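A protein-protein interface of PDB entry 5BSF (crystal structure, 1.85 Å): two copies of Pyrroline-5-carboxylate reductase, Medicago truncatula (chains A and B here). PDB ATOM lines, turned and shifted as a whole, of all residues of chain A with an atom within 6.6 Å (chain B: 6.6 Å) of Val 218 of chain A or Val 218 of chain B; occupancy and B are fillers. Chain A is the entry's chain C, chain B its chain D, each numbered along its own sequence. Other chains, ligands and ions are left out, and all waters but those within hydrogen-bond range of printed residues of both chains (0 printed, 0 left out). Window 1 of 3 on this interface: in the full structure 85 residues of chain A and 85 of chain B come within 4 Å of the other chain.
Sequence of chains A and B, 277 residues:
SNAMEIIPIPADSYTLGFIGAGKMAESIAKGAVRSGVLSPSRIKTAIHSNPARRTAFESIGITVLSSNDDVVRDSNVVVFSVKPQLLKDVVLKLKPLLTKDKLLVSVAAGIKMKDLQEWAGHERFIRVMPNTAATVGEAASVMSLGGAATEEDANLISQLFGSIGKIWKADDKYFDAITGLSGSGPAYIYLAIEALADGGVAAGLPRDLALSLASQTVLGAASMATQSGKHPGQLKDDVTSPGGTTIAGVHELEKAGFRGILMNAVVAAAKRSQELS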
ATOM      1  N   GLY A 185      -6.795  10.853 -15.656  1.00  0.00           N
ATOM      2  CA  GLY A 185      -6.424  11.661 -16.780  1.00  0.00           C
ATOM      3  C   GLY A 185      -5.009  11.508 -17.293  1.00  0.00           C
ATOM      4  O   GLY A 185      -4.769  11.627 -18.468  1.00  0.00           O
ATOM      5  N   PRO A 186      -4.008  11.319 -16.391  1.00  0.00           N
ATOM      6  CA  PRO A 186      -2.678  11.216 -16.933  1.00  0.00           C
ATOM      7  C   PRO A 186      -2.568  10.126 -17.975  1.00  0.00           C
ATOM      8  O   PRO A 186      -1.837  10.284 -18.985  1.00  0.00           O
ATOM      9  CB  PRO A 186      -1.804  10.911 -15.717  1.00  0.00           C
ATOM     10  CG  PRO A 186      -2.539  11.607 -14.615  1.00  0.00           C
ATOM     11  CD  PRO A 186      -3.995  11.361 -14.923  1.00  0.00           C
ATOM     12  N   ILE A 189      -3.529  11.339 -21.391  1.00  0.00           N
ATOM     13  CA  ILE A 189      -2.430  12.133 -21.941  1.00  0.00           C
ATOM     14  C   ILE A 189      -1.233  11.314 -22.409  1.00  0.00           C
ATOM     15  O   ILE A 189      -0.615  11.645 -23.389  1.00  0.00           O
ATOM     16  CB  ILE A 189      -2.058  13.230 -20.965  1.00  0.00           C
ATOM     17  CG1 ILE A 189      -3.302  14.081 -20.656  1.00  0.00           C
ATOM     18  CG2 ILE A 189      -0.971  14.128 -21.547  1.00  0.00           C
ATOM     19  CD1 ILE A 189      -4.089  14.607 -21.879  1.00  0.00           C
ATOM     20  N   ALA A 192      -2.264  10.228 -25.686  1.00  0.00           N
ATOM     21  CA  ALA A 192      -2.200  11.320 -26.587  1.00  0.00           C
ATOM     22  C   ALA A 192      -0.772  11.593 -27.047  1.00  0.00           C
ATOM     23  O   ALA A 192      -0.536  11.914 -28.214  1.00  0.00           O
ATOM     24  CB  ALA A 192      -2.756  12.609 -25.940  1.00  0.00           C
ATOM     25  N   ILE A 193       0.147  11.577 -26.115  1.00  0.00           N
ATOM     26  CA  ILE A 193       1.597  11.791 -26.428  1.00  0.00           C
ATOM     27  C   ILE A 193       2.118  10.750 -27.381  1.00  0.00           C
ATOM     28  O   ILE A 193       2.777  11.091 -28.390  1.00  0.00           O
ATOM     29  CB  ILE A 193       2.470  11.882 -25.155  1.00  0.00           C
ATOM     30  CG1 ILE A 193       2.179  13.237 -24.439  1.00  0.00           C
ATOM     31  CG2 ILE A 193       3.949  11.729 -25.523  1.00  0.00           C
ATOM     32  CD1 ILE A 193       2.711  13.276 -23.043  1.00  0.00           C
ATOM     33  N   LEU A 196       0.454  11.391 -30.856  1.00  0.00           N
ATOM     34  CA  LEU A 196       1.103  12.516 -31.501  1.00  0.00           C
ATOM     35  C   LEU A 196       2.451  12.167 -32.098  1.00  0.00           C
ATOM     36  O   LEU A 196       2.758  12.530 -33.232  1.00  0.00           O
ATOM     37  CB  LEU A 196       1.211  13.696 -30.530  1.00  0.00           C
ATOM     38  CG  LEU A 196      -0.105  14.401 -30.175  1.00  0.00           C
ATOM     39  CD1 LEU A 196       0.154  15.370 -29.016  1.00  0.00           C
ATOM     40  CD2 LEU A 196      -0.631  15.189 -31.341  1.00  0.00           C
ATOM     41  N   LEU A 213       9.261  16.075 -29.346  1.00  0.00           N
ATOM     42  CA  LEU A 213       8.348  17.200 -29.696  1.00  0.00           C
ATOM     43  C   LEU A 213       6.969  17.008 -29.122  1.00  0.00           C
ATOM     44  O   LEU A 213       6.345  17.942 -28.601  1.00  0.00           O
ATOM     45  CB  LEU A 213       8.242  17.420 -31.198  1.00  0.00           C
ATOM     46  CG  LEU A 213       9.528  17.916 -31.893  1.00  0.00           C
ATOM     47  CD1 LEU A 213       9.298  17.972 -33.395  1.00  0.00           C
ATOM     48  CD2 LEU A 213       9.923  19.278 -31.394  1.00  0.00           C
ATOM     49  N   ALA A 214       6.463  15.774 -29.211  1.00  0.00           N
ATOM     50  CA  ALA A 214       5.123  15.470 -28.630  1.00  0.00           C
ATOM     51  C   ALA A 214       5.009  15.789 -27.167  1.00  0.00           C
ATOM     52  O   ALA A 214       4.148  16.566 -26.732  1.00  0.00           O
ATOM     53  CB  ALA A 214       4.707  14.022 -28.891  1.00  0.00           C
ATOM     54  N   SER A 215       5.977  15.336 -26.406  1.00  0.00           N
ATOM     55  CA  SER A 215       5.947  15.599 -24.933  1.00  0.00           C
ATOM     56  C   SER A 215       6.096  17.057 -24.564  1.00  0.00           C
ATOM     57  O   SER A 215       5.350  17.579 -23.763  1.00  0.00           O
ATOM     58  CB  SER A 215       7.069  14.772 -24.232  1.00  0.00           C
ATOM     59  OG  SER A 215       6.777  13.424 -24.346  1.00  0.00           O
ATOM     60  N   GLN A 216       6.994  17.763 -25.261  1.00  0.00           N
ATOM     61  CA  GLN A 216       7.235  19.128 -24.905  1.00  0.00           C
ATOM     62  C   GLN A 216       6.083  20.028 -25.415  1.00  0.00           C
ATOM     63  O   GLN A 216       5.783  21.029 -24.846  1.00  0.00           O
ATOM     64  CB  GLN A 216       8.571  19.582 -25.492  1.00  0.00           C
ATOM     65  CG  GLN A 216       8.936  21.040 -25.159  1.00  0.00           C
ATOM     66  CD  GLN A 216       9.127  21.296 -23.671  1.00  0.00           C
ATOM     67  OE1 GLN A 216       9.520  20.441 -22.938  1.00  0.00           O
ATOM     68  NE2 GLN A 216       8.746  22.476 -23.240  1.00  0.00           N
ATOM     69  N   THR A 217       5.460  19.603 -26.530  1.00  0.00           N
ATOM     70  CA  THR A 217       4.301  20.315 -27.063  1.00  0.00           C
ATOM     71  C   THR A 217       3.174  20.278 -26.074  1.00  0.00           C
ATOM     72  O   THR A 217       2.512  21.318 -25.755  1.00  0.00           O
ATOM     73  CB  THR A 217       3.909  19.785 -28.434  1.00  0.00           C
ATOM     74  OG1 THR A 217       4.963  20.069 -29.350  1.00  0.00           O
ATOM     75  CG2 THR A 217       2.667  20.483 -28.987  1.00  0.00           C
ATOM     76  N   VAL A 218       2.898  19.098 -25.557  1.00  0.00           N
ATOM     77  CA  VAL A 218       1.831  18.961 -24.560  1.00  0.00           C
ATOM     78  C   VAL A 218       2.158  19.745 -23.290  1.00  0.00           C
ATOM     79  O   VAL A 218       1.346  20.482 -22.756  1.00  0.00           O
ATOM     80  CB  VAL A 218       1.574  17.465 -24.225  1.00  0.00           C
ATOM     81  CG1 VAL A 218       0.500  17.343 -23.172  1.00  0.00           C
ATOM     82  CG2 VAL A 218       1.154  16.737 -25.455  1.00  0.00           C
ATOM     83  N   LEU A 219       3.407  19.622 -22.839  1.00  0.00           N
ATOM     84  CA  LEU A 219       3.875  20.397 -21.637  1.00  0.00           C
ATOM     85  C   LEU A 219       3.681  21.928 -21.808  1.00  0.00           C
ATOM     86  O   LEU A 219       3.132  22.625 -20.973  1.00  0.00           O
ATOM     87  CB  LEU A 219       5.291  20.040 -21.302  1.00  0.00           C
ATOM     88  CG  LEU A 219       6.029  20.873 -20.192  1.00  0.00           C
ATOM     89  CD1 LEU A 219       5.184  20.685 -19.028  1.00  0.00           C
ATOM     90  CD2 LEU A 219       7.387  20.217 -19.845  1.00  0.00           C
ATOM     91  N   GLY A 220       4.118  22.424 -22.951  1.00  0.00           N
ATOM     92  CA  GLY A 220       4.024  23.814 -23.256  1.00  0.00           C
ATOM     93  C   GLY A 220       2.625  24.324 -23.367  1.00  0.00           C
ATOM     94  O   GLY A 220       2.283  25.369 -22.801  1.00  0.00           O
ATOM     95  N   ALA A 221       1.768  23.556 -24.016  1.00  0.00           N
ATOM     96  CA  ALA A 221       0.358  23.954 -24.163  1.00  0.00           C
ATOM     97  C   ALA A 221      -0.330  23.989 -22.783  1.00  0.00           C
ATOM     98  O   ALA A 221      -1.067  24.941 -22.441  1.00  0.00           O
ATOM     99  CB  ALA A 221      -0.376  22.994 -25.077  1.00  0.00           C
ATOM    100  N   ALA A 222      -0.028  22.997 -21.965  1.00  0.00           N
ATOM    101  CA  ALA A 222      -0.605  22.989 -20.593  1.00  0.00           C
ATOM    102  C   ALA A 222      -0.074  24.136 -19.728  1.00  0.00           C
ATOM    103  O   ALA A 222      -0.839  24.725 -18.950  1.00  0.00           O
ATOM    104  CB  ALA A 222      -0.372  21.683 -19.915  1.00  0.00           C
ATOM    105  N   SER A 223       1.182  24.515 -19.932  1.00  0.00           N
ATOM    106  CA  SER A 223       1.745  25.615 -19.211  1.00  0.00           C
ATOM    107  C   SER A 223       1.107  26.932 -19.607  1.00  0.00           C
ATOM    108  O   SER A 223       0.913  27.829 -18.776  1.00  0.00           O
ATOM    109  CB  SER A 223       3.283  25.732 -19.395  1.00  0.00           C
ATOM    110  OG  SER A 223       3.890  24.512 -19.037  1.00  0.00           O
ATOM    111  N   GLY B 185       0.237  21.436 -32.694  1.00  0.00           N
ATOM    112  CA  GLY B 185      -0.204  20.611 -31.606  1.00  0.00           C
ATOM    113  C   GLY B 185      -0.718  21.293 -30.356  1.00  0.00           C
ATOM    114  O   GLY B 185      -1.638  20.781 -29.698  1.00  0.00           O
ATOM    115  N   PRO B 186      -0.254  22.505 -30.043  1.00  0.00           N
ATOM    116  CA  PRO B 186      -0.879  23.142 -28.859  1.00  0.00           C
ATOM    117  C   PRO B 186      -2.401  23.293 -28.946  1.00  0.00           C
ATOM    118  O   PRO B 186      -3.109  23.123 -27.975  1.00  0.00           O
ATOM    119  CB  PRO B 186      -0.205  24.531 -28.801  1.00  0.00           C
ATOM    120  CG  PRO B 186       1.163  24.248 -29.401  1.00  0.00           C
ATOM    121  CD  PRO B 186       0.874  23.280 -30.535  1.00  0.00           C
ATOM    122  N   ILE B 189      -4.153  20.218 -27.831  1.00  0.00           N
ATOM    123  CA  ILE B 189      -4.188  20.163 -26.412  1.00  0.00           C
ATOM    124  C   ILE B 189      -5.135  21.136 -25.754  1.00  0.00           C
ATOM    125  O   ILE B 189      -5.730  20.837 -24.730  1.00  0.00           O
ATOM    126  CB  ILE B 189      -2.738  20.290 -25.884  1.00  0.00           C
ATOM    127  CG1 ILE B 189      -1.888  19.173 -26.512  1.00  0.00           C
ATOM    128  CG2 ILE B 189      -2.711  20.176 -24.388  1.00  0.00           C
ATOM    129  CD1 ILE B 189      -2.422  17.752 -26.399  1.00  0.00           C
ATOM    130  N   ALA B 192      -8.226  19.355 -25.885  1.00  0.00           N
ATOM    131  CA  ALA B 192      -8.260  18.324 -24.926  1.00  0.00           C
ATOM    132  C   ALA B 192      -8.539  18.822 -23.530  1.00  0.00           C
ATOM    133  O   ALA B 192      -9.251  18.193 -22.775  1.00  0.00           O
ATOM    134  CB  ALA B 192      -6.942  17.566 -24.935  1.00  0.00           C
ATOM    135  N   ILE B 193      -7.912  19.940 -23.180  1.00  0.00           N
ATOM    136  CA  ILE B 193      -8.141  20.546 -21.853  1.00  0.00           C
ATOM    137  C   ILE B 193      -9.587  20.939 -21.657  1.00  0.00           C
ATOM    138  O   ILE B 193     -10.170  20.659 -20.609  1.00  0.00           O
ATOM    139  CB  ILE B 193      -7.180  21.726 -21.617  1.00  0.00           C
ATOM    140  CG1 ILE B 193      -5.747  21.132 -21.369  1.00  0.00           C
ATOM    141  CG2 ILE B 193      -7.619  22.563 -20.435  1.00  0.00           C
ATOM    142  CD1 ILE B 193      -4.674  22.194 -21.401  1.00  0.00           C
ATOM    143  N   LEU B 196     -11.708  17.743 -21.390  1.00  0.00           N
ATOM    144  CA  LEU B 196     -11.534  17.154 -20.046  1.00  0.00           C
ATOM    145  C   LEU B 196     -12.329  17.897 -18.982  1.00  0.00           C
ATOM    146  O   LEU B 196     -12.985  17.278 -18.135  1.00  0.00           O
ATOM    147  CB  LEU B 196     -10.030  17.052 -19.662  1.00  0.00           C
ATOM    148  CG  LEU B 196      -9.230  15.977 -20.449  1.00  0.00           C
ATOM    149  CD1 LEU B 196      -7.768  16.248 -20.160  1.00  0.00           C
ATOM    150  CD2 LEU B 196      -9.616  14.617 -20.035  1.00  0.00           C
ATOM    151  N   LEU B 213      -8.174  21.393 -12.654  1.00  0.00           N
ATOM    152  CA  LEU B 213      -7.665  20.045 -12.694  1.00  0.00           C
ATOM    153  C   LEU B 213      -7.256  19.589 -14.073  1.00  0.00           C
ATOM    154  O   LEU B 213      -6.248  18.870 -14.251  1.00  0.00           O
ATOM    155  CB  LEU B 213      -8.701  19.045 -12.126  1.00  0.00           C
ATOM    156  CG  LEU B 213      -8.988  19.194 -10.622  1.00  0.00           C
ATOM    157  CD1 LEU B 213     -10.088  18.211 -10.251  1.00  0.00           C
ATOM    158  CD2 LEU B 213      -7.756  18.935  -9.759  1.00  0.00           C
ATOM    159  N   ALA B 214      -8.054  19.944 -15.045  1.00  0.00           N
ATOM    160  CA  ALA B 214      -7.722  19.521 -16.455  1.00  0.00           C
ATOM    161  C   ALA B 214      -6.386  20.011 -16.889  1.00  0.00           C
ATOM    162  O   ALA B 214      -5.511  19.242 -17.308  1.00  0.00           O
ATOM    163  CB  ALA B 214      -8.773  19.950 -17.409  1.00  0.00           C
ATOM    164  N   SER B 215      -6.153  21.290 -16.675  1.00  0.00           N
ATOM    165  CA  SER B 215      -4.837  21.906 -17.077  1.00  0.00           C
ATOM    166  C   SER B 215      -3.664  21.334 -16.335  1.00  0.00           C
ATOM    167  O   SER B 215      -2.650  20.970 -16.915  1.00  0.00           O
ATOM    168  CB  SER B 215      -4.916  23.450 -16.861  1.00  0.00           C
ATOM    169  OG  SER B 215      -5.823  23.980 -17.766  1.00  0.00           O
ATOM    170  N   GLN B 216      -3.816  21.164 -15.017  1.00  0.00           N
ATOM    171  CA  GLN B 216      -2.685  20.672 -14.224  1.00  0.00           C
ATOM    172  C   GLN B 216      -2.456  19.163 -14.431  1.00  0.00           C
ATOM    173  O   GLN B 216      -1.332  18.704 -14.393  1.00  0.00           O
ATOM    174  CB  GLN B 216      -2.945  20.946 -12.752  1.00  0.00           C
ATOM    175  CG  GLN B 216      -1.801  20.510 -11.869  1.00  0.00           C
ATOM    176  CD  GLN B 216      -0.526  21.286 -12.149  1.00  0.00           C
ATOM    177  OE1 GLN B 216      -0.543  22.424 -12.510  1.00  0.00           O
ATOM    178  NE2 GLN B 216       0.593  20.630 -11.954  1.00  0.00           N
ATOM    179  N   THR B 217      -3.533  18.435 -14.727  1.00  0.00           N
ATOM    180  CA  THR B 217      -3.395  17.003 -15.115  1.00  0.00           C
ATOM    181  C   THR B 217      -2.574  16.834 -16.378  1.00  0.00           C
ATOM    182  O   THR B 217      -1.628  16.019 -16.451  1.00  0.00           O
ATOM    183  CB  THR B 217      -4.748  16.353 -15.194  1.00  0.00           C
ATOM    184  OG1 THR B 217      -5.367  16.397 -13.886  1.00  0.00           O
ATOM    185  CG2 THR B 217      -4.648  14.960 -15.614  1.00  0.00           C
ATOM    186  N   VAL B 218      -2.903  17.631 -17.379  1.00  0.00           N
ATOM    187  CA  VAL B 218      -2.156  17.596 -18.625  1.00  0.00           C
ATOM    188  C   VAL B 218      -0.684  18.011 -18.389  1.00  0.00           C
ATOM    189  O   VAL B 218       0.240  17.333 -18.855  1.00  0.00           O
ATOM    190  CB  VAL B 218      -2.803  18.418 -19.715  1.00  0.00           C
ATOM    191  CG1 VAL B 218      -2.020  18.404 -20.993  1.00  0.00           C
ATOM    192  CG2 VAL B 218      -4.210  17.933 -20.013  1.00  0.00           C
ATOM    193  N   LEU B 219      -0.495  19.072 -17.618  1.00  0.00           N
ATOM    194  CA  LEU B 219       0.855  19.554 -17.346  1.00  0.00           C
ATOM    195  C   LEU B 219       1.703  18.448 -16.630  1.00  0.00           C
ATOM    196  O   LEU B 219       2.832  18.151 -16.991  1.00  0.00           O
ATOM    197  CB  LEU B 219       0.796  20.823 -16.499  1.00  0.00           C
ATOM    198  CG  LEU B 219       2.145  21.383 -15.948  1.00  0.00           C
ATOM    199  CD1 LEU B 219       2.961  21.574 -17.115  1.00  0.00           C
ATOM    200  CD2 LEU B 219       1.938  22.789 -15.370  1.00  0.00           C
ATOM    201  N   GLY B 220       1.096  17.842 -15.611  1.00  0.00           N
ATOM    202  CA  GLY B 220       1.767  16.821 -14.852  1.00  0.00           C
ATOM    203  C   GLY B 220       2.088  15.573 -15.631  1.00  0.00           C
ATOM    204  O   GLY B 220       3.197  15.088 -15.569  1.00  0.00           O
ATOM    205  N   ALA B 221       1.145  15.131 -16.455  1.00  0.00           N
ATOM    206  CA  ALA B 221       1.390  13.982 -17.308  1.00  0.00           C
ATOM    207  C   ALA B 221       2.542  14.260 -18.311  1.00  0.00           C
ATOM    208  O   ALA B 221       3.445  13.426 -18.510  1.00  0.00           O
ATOM    209  CB  ALA B 221       0.121  13.605 -18.077  1.00  0.00           C
ATOM    210  N   ALA B 222       2.546  15.457 -18.892  1.00  0.00           N
ATOM    211  CA  ALA B 222       3.631  15.804 -19.855  1.00  0.00           C
ATOM    212  C   ALA B 222       4.956  15.873 -19.139  1.00  0.00           C
ATOM    213  O   ALA B 222       5.986  15.501 -19.693  1.00  0.00           O
ATOM    214  CB  ALA B 222       3.331  17.059 -20.560  1.00  0.00           C
ATOM    215  N   SER B 223       4.932  16.401 -17.911  1.00  0.00           N
ATOM    216  CA  SER B 223       6.158  16.481 -17.110  1.00  0.00           C
ATOM    217  C   SER B 223       6.722  15.100 -16.789  1.00  0.00           C
ATOM    218  O   SER B 223       7.959  14.884 -16.785  1.00  0.00           O
ATOM    219  CB  SER B 223       5.975  17.256 -15.835  1.00  0.00           C
ATOM    220  OG  SER B 223       5.471  18.547 -16.133  1.00  0.00           O
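The backbone carbonyl oxygen (O) of Leu 219 of chain A lies within hydrogen-bond range of the side-chain hydroxyl (OG) of Ser 223 of chain A (2.8 Å). The backbone carbonyl oxygen (O) of Leu 213 of chain B sits at hydrogen-bond distance from the side-chain hydroxyl (OG1) of Thr 217 of chain B (2.7 Å). The side-chain hydroxyl (OG1) of Thr 217 of chain A lies within hydrogen-bond range of the backbone carbonyl oxygen (O) of Leu 213 of chain A, at 2.6 Å. The backbone carbonyl oxygen (O) of Leu 219 of chain B sits at hydrogen-bond distance from the side-chain hydroxyl (OG) of Ser 223 of chain B.
Gly 185 of chain A touches Thr 217 of chain B, and with the chains exchanged Thr 217 of chain A touches Gly 185 of chain B. Pro 186 of chain A touches Thr 217 of chain B, and with the chains exchanged Thr 217 of chain A touches Pro 186 of chain B. Leu 219 of chain A touches its own counterpart, Leu 219 of chain B. Leu 219 of chain A touches Ser 223 of chain B, and with the chains exchanged Ser 223 of chain A touches Leu 219 of chain B. Positions printed for both chains: 185, 186, 189, 192, 193, 196, 213, 214, 215, 216, 217, 218, 219, 220, 221, 222 and 223. Of the 20 pairs that touch across the chains among the printed residues, 20 have their exchanged pair printed and touching as well.
Ala 192 of chain A touches none of the printed residues of chain B. Of chain B, only Ile 189, Val 218 and Ala 222 come within 4 Å of Val 218 of chain A. Of the printed residues of chain B, Ser 223 of chain A touches Leu 219. Of the printed residues of chain A, Ile 189 of chain B touches Val 218 (3.8 Å) and Ala 221 (3.7 Å). Of the printed residues of chain A, Thr 217 of chain B touches Gly 185 and Pro 186. Printed residues of chain A within 4 Å of Ala 221 of chain B: Pro 186 (3.9 Å) and Ile 189 (3.6 Å). Printed residues of chain A within 4 Å of Ser 223 of chain B: Leu 219 (3.6 Å).
Hydrophobic or aromatic side chains of chain A that line the printed part of chain B: Pro 186, Ile 189, Val 218, Leu 219, Ala 221 and Ala 222. Of the 17 printed residues of chain B, 10 touch a printed residue of chain A. Hydrophobic or aromatic side chains of chain B that line the printed part of chain A: Pro 186, Ile 189, Val 218, Leu 219, Ala 221 and Ala 222. Among the printed residues, no Asp or Glu carboxylate lies within 4 Å of a Lys or Arg side-chain nitrogen of the other chain.
Among the printed residues, merely in contact across the chains: Leu 219 of chain A with Leu 219 of chain B, Leu 219 of chain A with Ala 222 of chain B, Ala 222 of chain A with Leu 219 of chain B, Val 218 of chain A with Val 218 of chain B, Leu 219 of chain A with Ser 223 of chain B, Ser 223 of chain A with Leu 219 of chain B, Ile 189 of chain A with Ala 221 of chain B, Thr 217 of chain A with Pro 186 of chain B, Ala 221 of chain A with Ile 189 of chain B, Pro 186 of chain A with Thr 217 of chain B, Thr 217 of chain A with Gly 185 of chain B, Ile 189 of chain A with Val 218 of chain B, Ala 221 of chain A with Pro 186 of chain B, Ser 215 of chain A with Ala 222 of chain B, Ala 222 of chain A with Val 218 of chain B, Ala 222 of chain A with Ser 215 of chain B, Val 218 of chain A with Ile 189 of chain B, Pro 186 of chain A with Ala 221 of chain B, Gly 185 of chain A with Thr 217 of chain B and Val 218 of chain A with Ala 222 of chain B.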
